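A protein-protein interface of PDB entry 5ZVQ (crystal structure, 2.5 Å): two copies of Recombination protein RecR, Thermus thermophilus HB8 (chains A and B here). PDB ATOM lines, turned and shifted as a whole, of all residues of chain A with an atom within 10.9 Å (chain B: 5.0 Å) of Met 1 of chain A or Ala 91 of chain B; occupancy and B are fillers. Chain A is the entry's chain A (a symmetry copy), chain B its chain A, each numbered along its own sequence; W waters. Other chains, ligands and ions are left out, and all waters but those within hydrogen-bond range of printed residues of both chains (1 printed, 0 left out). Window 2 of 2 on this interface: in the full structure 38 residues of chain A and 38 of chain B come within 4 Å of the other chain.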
ATOM      1  N   MET A   1     -16.965 -15.301  17.228  1.00  0.00           N
ATOM      2  CA  MET A   1     -17.020 -15.358  15.727  1.00  0.00           C
ATOM      3  C   MET A   1     -15.711 -15.849  15.100  1.00  0.00           C
ATOM      4  O   MET A   1     -15.699 -16.876  14.414  1.00  0.00           O
ATOM      5  CB  MET A   1     -17.417 -13.990  15.128  1.00  0.00           C
ATOM      6  CG  MET A   1     -18.925 -13.760  15.041  1.00  0.00           C
ATOM      7  SD  MET A   1     -19.488 -12.271  14.184  1.00  0.00           S
ATOM      8  CE  MET A   1     -21.269 -12.379  14.393  1.00  0.00           C
ATOM      9  N   ARG A   2     -14.621 -15.119  15.341  1.00  0.00           N
ATOM     10  CA  ARG A   2     -13.352 -15.343  14.638  1.00  0.00           C
ATOM     11  C   ARG A   2     -12.580 -16.574  15.115  1.00  0.00           C
ATOM     12  O   ARG A   2     -12.787 -17.058  16.229  1.00  0.00           O
ATOM     13  CB  ARG A   2     -12.454 -14.106  14.752  1.00  0.00           C
ATOM     14  N   TYR A   3     -11.705 -17.066  14.231  1.00  0.00           N
ATOM     15  CA  TYR A   3     -10.850 -18.244  14.474  1.00  0.00           C
ATOM     16  C   TYR A   3      -9.336 -18.129  14.125  1.00  0.00           C
ATOM     17  O   TYR A   3      -8.525 -18.707  14.850  1.00  0.00           O
ATOM     18  CB  TYR A   3     -11.462 -19.486  13.800  1.00  0.00           C
ATOM     19  CG  TYR A   3     -12.751 -19.951  14.455  1.00  0.00           C
ATOM     20  CD1 TYR A   3     -12.733 -20.716  15.624  1.00  0.00           C
ATOM     21  CD2 TYR A   3     -14.000 -19.612  13.914  1.00  0.00           C
ATOM     22  CE1 TYR A   3     -13.915 -21.131  16.231  1.00  0.00           C
ATOM     23  CE2 TYR A   3     -15.188 -20.029  14.515  1.00  0.00           C
ATOM     24  CZ  TYR A   3     -15.141 -20.786  15.670  1.00  0.00           C
ATOM     25  OH  TYR A   3     -16.321 -21.195  16.253  1.00  0.00           O
ATOM     26  N   PRO A   4      -8.941 -17.417  13.036  1.00  0.00           N
ATOM     27  CA  PRO A   4      -7.486 -17.232  12.854  1.00  0.00           C
ATOM     28  C   PRO A   4      -6.838 -16.463  14.008  1.00  0.00           C
ATOM     29  O   PRO A   4      -7.443 -15.517  14.530  1.00  0.00           O
ATOM     30  CB  PRO A   4      -7.390 -16.427  11.552  1.00  0.00           C
ATOM     31  CG  PRO A   4      -8.630 -16.755  10.815  1.00  0.00           C
ATOM     32  CD  PRO A   4      -9.683 -16.890  11.873  1.00  0.00           C
ATOM     33  N   GLU A   5      -5.625 -16.865  14.388  1.00  0.00           N
ATOM     34  CA  GLU A   5      -5.010 -16.392  15.641  1.00  0.00           C
ATOM     35  C   GLU A   5      -4.587 -14.923  15.615  1.00  0.00           C
ATOM     36  O   GLU A   5      -4.897 -14.176  16.546  1.00  0.00           O
ATOM     37  CB  GLU A   5      -3.824 -17.285  16.067  1.00  0.00           C
ATOM     38  CG  GLU A   5      -4.197 -18.387  17.054  1.00  0.00           C
ATOM     39  CD  GLU A   5      -4.749 -17.845  18.368  1.00  0.00           C
ATOM     40  OE1 GLU A   5      -5.850 -18.275  18.777  1.00  0.00           O
ATOM     41  OE2 GLU A   5      -4.100 -16.969  18.980  1.00  0.00           O
ATOM     42  N   LEU A   7      -5.691 -12.596  13.615  1.00  0.00           N
ATOM     43  CA  LEU A   7      -6.939 -11.840  13.571  1.00  0.00           C
ATOM     44  C   LEU A   7      -7.530 -11.677  14.967  1.00  0.00           C
ATOM     45  O   LEU A   7      -7.901 -10.575  15.359  1.00  0.00           O
ATOM     46  CB  LEU A   7      -7.962 -12.519  12.657  1.00  0.00           C
ATOM     47  CG  LEU A   7      -9.259 -11.739  12.420  1.00  0.00           C
ATOM     48  CD1 LEU A   7      -8.992 -10.469  11.617  1.00  0.00           C
ATOM     49  CD2 LEU A   7     -10.289 -12.613  11.725  1.00  0.00           C
ATOM     50  N   LEU A   8      -7.617 -12.775  15.711  1.00  0.00           N
ATOM     51  CA  LEU A   8      -8.149 -12.730  17.074  1.00  0.00           C
ATOM     52  C   LEU A   8      -7.244 -11.916  18.008  1.00  0.00           C
ATOM     53  O   LEU A   8      -7.731 -11.152  18.840  1.00  0.00           O
ATOM     54  CB  LEU A   8      -8.350 -14.149  17.616  1.00  0.00           C
ATOM     55  CG  LEU A   8      -9.224 -14.289  18.864  1.00  0.00           C
ATOM     56  CD1 LEU A   8     -10.666 -13.872  18.586  1.00  0.00           C
ATOM     57  CD2 LEU A   8      -9.156 -15.725  19.359  1.00  0.00           C
ATOM     58  N   LYS A   9      -5.930 -12.085  17.851  1.00  0.00           N
ATOM     59  CA  LYS A   9      -4.922 -11.297  18.566  1.00  0.00           C
ATOM     60  C   LYS A   9      -5.093  -9.789  18.328  1.00  0.00           C
ATOM     61  O   LYS A   9      -4.928  -8.997  19.253  1.00  0.00           O
ATOM     62  CB  LYS A   9      -3.513 -11.741  18.139  1.00  0.00           C
ATOM     63  CG  LYS A   9      -2.364 -11.063  18.875  1.00  0.00           C
ATOM     64  N   THR A  11      -8.055  -8.320  17.101  1.00  0.00           N
ATOM     65  CA  THR A  11      -9.393  -8.023  17.628  1.00  0.00           C
ATOM     66  C   THR A  11      -9.393  -7.861  19.147  1.00  0.00           C
ATOM     67  O   THR A  11     -10.093  -6.999  19.681  1.00  0.00           O
ATOM     68  CB  THR A  11     -10.401  -9.129  17.246  1.00  0.00           C
ATOM     69  OG1 THR A  11     -10.372  -9.339  15.829  1.00  0.00           O
ATOM     70  CG2 THR A  11     -11.827  -8.755  17.665  1.00  0.00           C
ATOM     71  N   ARG A  12      -8.595  -8.682  19.828  1.00  0.00           N
ATOM     72  CA  ARG A  12      -8.476  -8.624  21.288  1.00  0.00           C
ATOM     73  C   ARG A  12      -7.733  -7.364  21.738  1.00  0.00           C
ATOM     74  O   ARG A  12      -8.148  -6.701  22.691  1.00  0.00           O
ATOM     75  CB  ARG A  12      -7.780  -9.883  21.811  1.00  0.00           C
ATOM     76  CG  ARG A  12      -8.072 -10.218  23.268  1.00  0.00           C
ATOM     77  CD  ARG A  12      -8.537 -11.662  23.405  1.00  0.00           C
ATOM     78  NE  ARG A  12      -7.576 -12.610  22.826  1.00  0.00           N
ATOM     79  CZ  ARG A  12      -7.854 -13.863  22.449  1.00  0.00           C
ATOM     80  NH1 ARG A  12      -9.084 -14.373  22.568  1.00  0.00           N
ATOM     81  NH2 ARG A  12      -6.883 -14.618  21.936  1.00  0.00           N
ATOM     82  N   PRO A  22     -16.686  -5.225  21.357  1.00  0.00           N
ATOM     83  CA  PRO A  22     -16.202  -6.323  20.504  1.00  0.00           C
ATOM     84  C   PRO A  22     -16.704  -6.298  19.057  1.00  0.00           C
ATOM     85  O   PRO A  22     -16.026  -6.825  18.178  1.00  0.00           O
ATOM     86  CB  PRO A  22     -16.701  -7.586  21.228  1.00  0.00           C
ATOM     87  CG  PRO A  22     -17.032  -7.146  22.613  1.00  0.00           C
ATOM     88  CD  PRO A  22     -17.517  -5.736  22.463  1.00  0.00           C
ATOM     89  N   LYS A  23     -17.863  -5.686  18.814  1.00  0.00           N
ATOM     90  CA  LYS A  23     -18.438  -5.628  17.465  1.00  0.00           C
ATOM     91  C   LYS A  23     -17.647  -4.675  16.573  1.00  0.00           C
ATOM     92  O   LYS A  23     -17.422  -4.964  15.394  1.00  0.00           O
ATOM     93  CB  LYS A  23     -19.917  -5.208  17.506  1.00  0.00           C
ATOM     94  CG  LYS A  23     -20.817  -6.027  16.596  1.00  0.00           C
ATOM     95  CD  LYS A  23     -21.129  -7.380  17.217  1.00  0.00           C
ATOM     96  CE  LYS A  23     -21.997  -8.233  16.305  1.00  0.00           C
ATOM     97  NZ  LYS A  23     -22.321  -9.542  16.937  1.00  0.00           N
ATOM     98  N   THR A  24     -17.242  -3.538  17.139  1.00  0.00           N
ATOM     99  CA  THR A  24     -16.377  -2.586  16.442  1.00  0.00           C
ATOM    100  C   THR A  24     -14.958  -3.139  16.282  1.00  0.00           C
ATOM    101  O   THR A  24     -14.356  -3.010  15.218  1.00  0.00           O
ATOM    102  CB  THR A  24     -16.328  -1.235  17.173  1.00  0.00           C
ATOM    103  OG1 THR A  24     -17.660  -0.726  17.302  1.00  0.00           O
ATOM    104  N   ALA A  25     -14.440  -3.764  17.336  1.00  0.00           N
ATOM    105  CA  ALA A  25     -13.146  -4.449  17.284  1.00  0.00           C
ATOM    106  C   ALA A  25     -13.032  -5.415  16.096  1.00  0.00           C
ATOM    107  O   ALA A  25     -12.010  -5.432  15.409  1.00  0.00           O
ATOM    108  CB  ALA A  25     -12.891  -5.194  18.583  1.00  0.00           C
ATOM    109  N   GLN A  26     -14.086  -6.193  15.852  1.00  0.00           N
ATOM    110  CA  GLN A  26     -14.105  -7.147  14.741  1.00  0.00           C
ATOM    111  C   GLN A  26     -14.142  -6.455  13.380  1.00  0.00           C
ATOM    112  O   GLN A  26     -13.379  -6.817  12.487  1.00  0.00           O
ATOM    113  CB  GLN A  26     -15.290  -8.101  14.864  1.00  0.00           C
ATOM    114  CG  GLN A  26     -15.336  -9.176  13.791  1.00  0.00           C
ATOM    115  CD  GLN A  26     -16.504 -10.116  13.976  1.00  0.00           C
ATOM    116  OE1 GLN A  26     -16.497 -10.951  14.879  1.00  0.00           O
ATOM    117  NE2 GLN A  26     -17.517  -9.988  13.114  1.00  0.00           N
ATOM    118  N   ARG A  27     -15.033  -5.476  13.224  1.00  0.00           N
ATOM    119  CA  ARG A  27     -15.155  -4.732  11.964  1.00  0.00           C
ATOM    120  C   ARG A  27     -13.833  -4.084  11.562  1.00  0.00           C
ATOM    121  O   ARG A  27     -13.474  -4.083  10.383  1.00  0.00           O
ATOM    122  CB  ARG A  27     -16.243  -3.655  12.062  1.00  0.00           C
ATOM    123  CG  ARG A  27     -16.605  -3.000  10.729  1.00  0.00           C
ATOM    124  CD  ARG A  27     -17.459  -1.750  10.901  1.00  0.00           C
ATOM    125  NE  ARG A  27     -18.694  -2.020  11.651  1.00  0.00           N
ATOM    126  CZ  ARG A  27     -18.954  -1.651  12.912  1.00  0.00           C
ATOM    127  NH1 ARG A  27     -18.078  -0.958  13.648  1.00  0.00           N
ATOM    128  NH2 ARG A  27     -20.129  -1.977  13.451  1.00  0.00           N
ATOM    129  N   ALA A  29     -10.724  -4.959  12.761  1.00  0.00           N
ATOM    130  CA  ALA A  29      -9.757  -6.039  12.563  1.00  0.00           C
ATOM    131  C   ALA A  29      -9.866  -6.628  11.160  1.00  0.00           C
ATOM    132  O   ALA A  29      -8.851  -6.819  10.486  1.00  0.00           O
ATOM    133  CB  ALA A  29      -9.957  -7.127  13.609  1.00  0.00           C
ATOM    134  N   LEU A  30     -11.097  -6.910  10.731  1.00  0.00           N
ATOM    135  CA  LEU A  30     -11.372  -7.373   9.360  1.00  0.00           C
ATOM    136  C   LEU A  30     -10.892  -6.362   8.337  1.00  0.00           C
ATOM    137  O   LEU A  30     -10.220  -6.722   7.372  1.00  0.00           O
ATOM    138  CB  LEU A  30     -12.873  -7.631   9.142  1.00  0.00           C
ATOM    139  CG  LEU A  30     -13.414  -9.047   9.363  1.00  0.00           C
ATOM    140  CD1 LEU A  30     -12.752  -9.737  10.545  1.00  0.00           C
ATOM    141  CD2 LEU A  30     -14.926  -9.011   9.539  1.00  0.00           C
ATOM    142  N   ALA B  87     -17.551 -11.024   7.299  1.00  0.00           N
ATOM    143  CA  ALA B  87     -18.462 -10.669   8.401  1.00  0.00           C
ATOM    144  C   ALA B  87     -19.772 -11.475   8.377  1.00  0.00           C
ATOM    145  O   ALA B  87     -20.257 -11.895   9.432  1.00  0.00           O
ATOM    146  CB  ALA B  87     -18.759  -9.179   8.389  1.00  0.00           C
ATOM    147  N   ASP B  88     -20.321 -11.697   7.180  1.00  0.00           N
ATOM    148  CA  ASP B  88     -21.552 -12.493   7.014  1.00  0.00           C
ATOM    149  C   ASP B  88     -21.345 -13.982   7.268  1.00  0.00           C
ATOM    150  O   ASP B  88     -22.237 -14.655   7.785  1.00  0.00           O
ATOM    151  CB  ASP B  88     -22.126 -12.324   5.605  1.00  0.00           C
ATOM    152  CG  ASP B  88     -22.686 -10.939   5.351  1.00  0.00           C
ATOM    153  OD1 ASP B  88     -22.964 -10.192   6.315  1.00  0.00           O
ATOM    154  OD2 ASP B  88     -22.864 -10.606   4.165  1.00  0.00           O
ATOM    155  N   LEU B  89     -20.184 -14.488   6.852  1.00  0.00           N
ATOM    156  CA  LEU B  89     -19.778 -15.868   7.098  1.00  0.00           C
ATOM    157  C   LEU B  89     -19.724 -16.114   8.600  1.00  0.00           C
ATOM    158  O   LEU B  89     -20.321 -17.071   9.087  1.00  0.00           O
ATOM    159  CB  LEU B  89     -18.409 -16.138   6.445  1.00  0.00           C
ATOM    160  CG  LEU B  89     -17.811 -17.552   6.460  1.00  0.00           C
ATOM    161  CD1 LEU B  89     -16.984 -17.786   5.208  1.00  0.00           C
ATOM    162  CD2 LEU B  89     -16.963 -17.813   7.700  1.00  0.00           C
ATOM    163  N   TYR B  90     -19.031 -15.235   9.328  1.00  0.00           N
ATOM    164  CA  TYR B  90     -18.961 -15.327  10.790  1.00  0.00           C
ATOM    165  C   TYR B  90     -20.337 -15.298  11.439  1.00  0.00           C
ATOM    166  O   TYR B  90     -20.594 -16.081  12.349  1.00  0.00           O
ATOM    167  CB  TYR B  90     -18.114 -14.201  11.391  1.00  0.00           C
ATOM    168  CG  TYR B  90     -16.628 -14.242  11.103  1.00  0.00           C
ATOM    169  CD1 TYR B  90     -16.007 -15.382  10.570  1.00  0.00           C
ATOM    170  CD2 TYR B  90     -15.821 -13.140  11.398  1.00  0.00           C
ATOM    171  CE1 TYR B  90     -14.643 -15.406  10.323  1.00  0.00           C
ATOM    172  CE2 TYR B  90     -14.454 -13.164  11.148  1.00  0.00           C
ATOM    173  CZ  TYR B  90     -13.875 -14.303  10.614  1.00  0.00           C
ATOM    174  OH  TYR B  90     -12.532 -14.361  10.361  1.00  0.00           O
ATOM    175  N   ALA B  91     -21.216 -14.406  10.979  1.00  0.00           N
ATOM    176  CA  ALA B  91     -22.580 -14.346  11.512  1.00  0.00           C
ATOM    177  C   ALA B  91     -23.292 -15.682  11.313  1.00  0.00           C
ATOM    178  O   ALA B  91     -23.826 -16.250  12.267  1.00  0.00           O
ATOM    179  CB  ALA B  91     -23.365 -13.215  10.869  1.00  0.00           C
ATOM    180  N   LEU B  92     -23.271 -16.179  10.075  1.00  0.00           N
ATOM    181  CA  LEU B  92     -23.836 -17.494   9.736  1.00  0.00           C
ATOM    182  C   LEU B  92     -23.278 -18.598  10.618  1.00  0.00           C
ATOM    183  O   LEU B  92     -24.030 -19.413  11.145  1.00  0.00           O
ATOM    184  CB  LEU B  92     -23.579 -17.854   8.261  1.00  0.00           C
ATOM    185  CG  LEU B  92     -24.728 -17.638   7.276  1.00  0.00           C
ATOM    186  CD1 LEU B  92     -25.072 -16.169   7.105  1.00  0.00           C
ATOM    187  CD2 LEU B  92     -24.371 -18.252   5.935  1.00  0.00           C
ATOM    188  N   GLU B  93     -21.957 -18.601  10.768  1.00  0.00           N
ATOM    189  CA  GLU B  93     -21.245 -19.610  11.540  1.00  0.00           C
ATOM    190  C   GLU B  93     -21.560 -19.502  13.033  1.00  0.00           C
ATOM    191  O   GLU B  93     -21.711 -20.524  13.709  1.00  0.00           O
ATOM    192  CB  GLU B  93     -19.732 -19.482  11.292  1.00  0.00           C
ATOM    193  CG  GLU B  93     -18.880 -20.645  11.779  1.00  0.00           C
ATOM    194  CD  GLU B  93     -19.317 -21.985  11.219  1.00  0.00           C
ATOM    195  OE1 GLU B  93     -19.200 -22.996  11.943  1.00  0.00           O
ATOM    196  OE2 GLU B  93     -19.784 -22.043  10.066  1.00  0.00           O
ATOM    197  N   ARG B  94     -21.664 -18.274  13.534  1.00  0.00           N
ATOM    198  CA  ARG B  94     -22.130 -18.026  14.906  1.00  0.00           C
ATOM    199  C   ARG B  94     -23.563 -18.518  15.180  1.00  0.00           C
ATOM    200  O   ARG B  94     -23.871 -18.882  16.317  1.00  0.00           O
ATOM    201  CB  ARG B  94     -22.032 -16.535  15.286  1.00  0.00           C
ATOM    202  CG  ARG B  94     -20.907 -16.199  16.254  1.00  0.00           C
ATOM    203  CD  ARG B  94     -21.263 -15.006  17.141  1.00  0.00           C
ATOM    204  NE  ARG B  94     -20.215 -14.729  18.130  1.00  0.00           N
ATOM    205  CZ  ARG B  94     -20.344 -13.932  19.195  1.00  0.00           C
ATOM    206  NH1 ARG B  94     -19.307 -13.761  20.012  1.00  0.00           N
ATOM    207  NH2 ARG B  94     -21.491 -13.307  19.464  1.00  0.00           N
ATOM    208  N   SER B  95     -24.428 -18.510  14.161  1.00  0.00           N
ATOM    209  CA  SER B  95     -25.821 -18.981  14.309  1.00  0.00           C
ATOM    210  C   SER B  95     -25.909 -20.437  14.774  1.00  0.00           C
ATOM    211  O   SER B  95     -26.860 -20.815  15.464  1.00  0.00           O
ATOM    212  CB  SER B  95     -26.625 -18.817  13.002  1.00  0.00           C
ATOM    213  OG  SER B  95     -26.355 -19.857  12.070  1.00  0.00           O
HETATM  214  O   HOH W   1     -20.047 -10.587  11.813  1.00  0.00           O
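Water W1 lies within hydrogen-bond range of the backbone carbonyl oxygen of Ala 87 of chain B (2.7 Å), the side-chain amide nitrogen of Gln 26 of chain A (2.9 Å) and the side-chain sulfur of Met 1 of chain A (3.0 Å).
The guanidinium group of Arg 94 of chain B lies close to the backbone NH of Met 1 of chain A (3.4 Å).
No position is printed for both chains.
Of the 7 pairs that touch across the chains among the printed residues, none has its exchanged pair printed and touching as well.
Of the 9 printed residues of chain B, 4 touch a printed residue of chain A.
Printed residues of chain B that touch a printed residue of chain A: Ala 87, Tyr 90, Ala 91 and Arg 94.
Hydrophobic or aromatic side chains of chain B within 4 Å of the printed part of chain A: Tyr 90.
Of the 18 printed residues of chain A, 4 touch a printed residue of chain B.
Printed residues of chain A that touch a printed residue of chain B: Met 1, Leu 7, Gln 26 and Leu 30.
Hydrophobic or aromatic side chains of chain A that line the printed part of chain B: Met 1, Leu 7 and Leu 30.
Among the printed residues, 7 pairs touch across the chains.
Among the printed residues, no Asp or Glu carboxylate lies within 4 Å of a Lys or Arg side-chain nitrogen of the other chain.
Among the printed residues, merely in contact across the chains: Met 1 of chain A with Tyr 90 of chain B (3.7 Å), Met 1 of chain A with Ala 91 of chain B (3.7 Å), Leu 7 of chain A with Tyr 90 of chain B (3.2 Å), Gln 26 of chain A with Tyr 90 of chain B (3.97 Å), Leu 30 of chain A with Ala 87 of chain B (3.995 Å) and Leu 30 of chain A with Tyr 90 of chain B (3.9 Å).
OG1 of Thr 11 of chain A sits at hydrogen-bond distance from O of Leu 7 of chain A (2.8 Å).
NE2 of Gln 26 of chain A lies within hydrogen-bond range of SD of Met 1 of chain A, 3.2 Å away.
Of chain B, only Tyr 90 (3.7 Å), Ala 91 (3.7 Å) and Arg 94 (3.4 Å) come within 4 Å of Met 1 of chain A.
Ala 91 of chain B touches one residue of chain A.
Leu 92 of chain B touches none of the printed residues of chain A.
Of chain A, only Met 1 (3.4 Å) comes within 4 Å of Arg 94 of chain B.
No residue of chain A comes within 4 Å of Ser 95 of chain B.
Of the printed residues of chain B, Gln 26 of chain A touches Tyr 90.
Printed residues of chain B within 4 Å of Leu 7 of chain A: Tyr 90.
Of the printed residues of chain B, Leu 30 of chain A touches Ala 87 and Tyr 90.
Pro 4 of chain A touches none of the printed residues of chain B.
The nearest residue of chain B that does not touch Met 1 of chain A is Ala 87 of chain B (4.8 Å).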
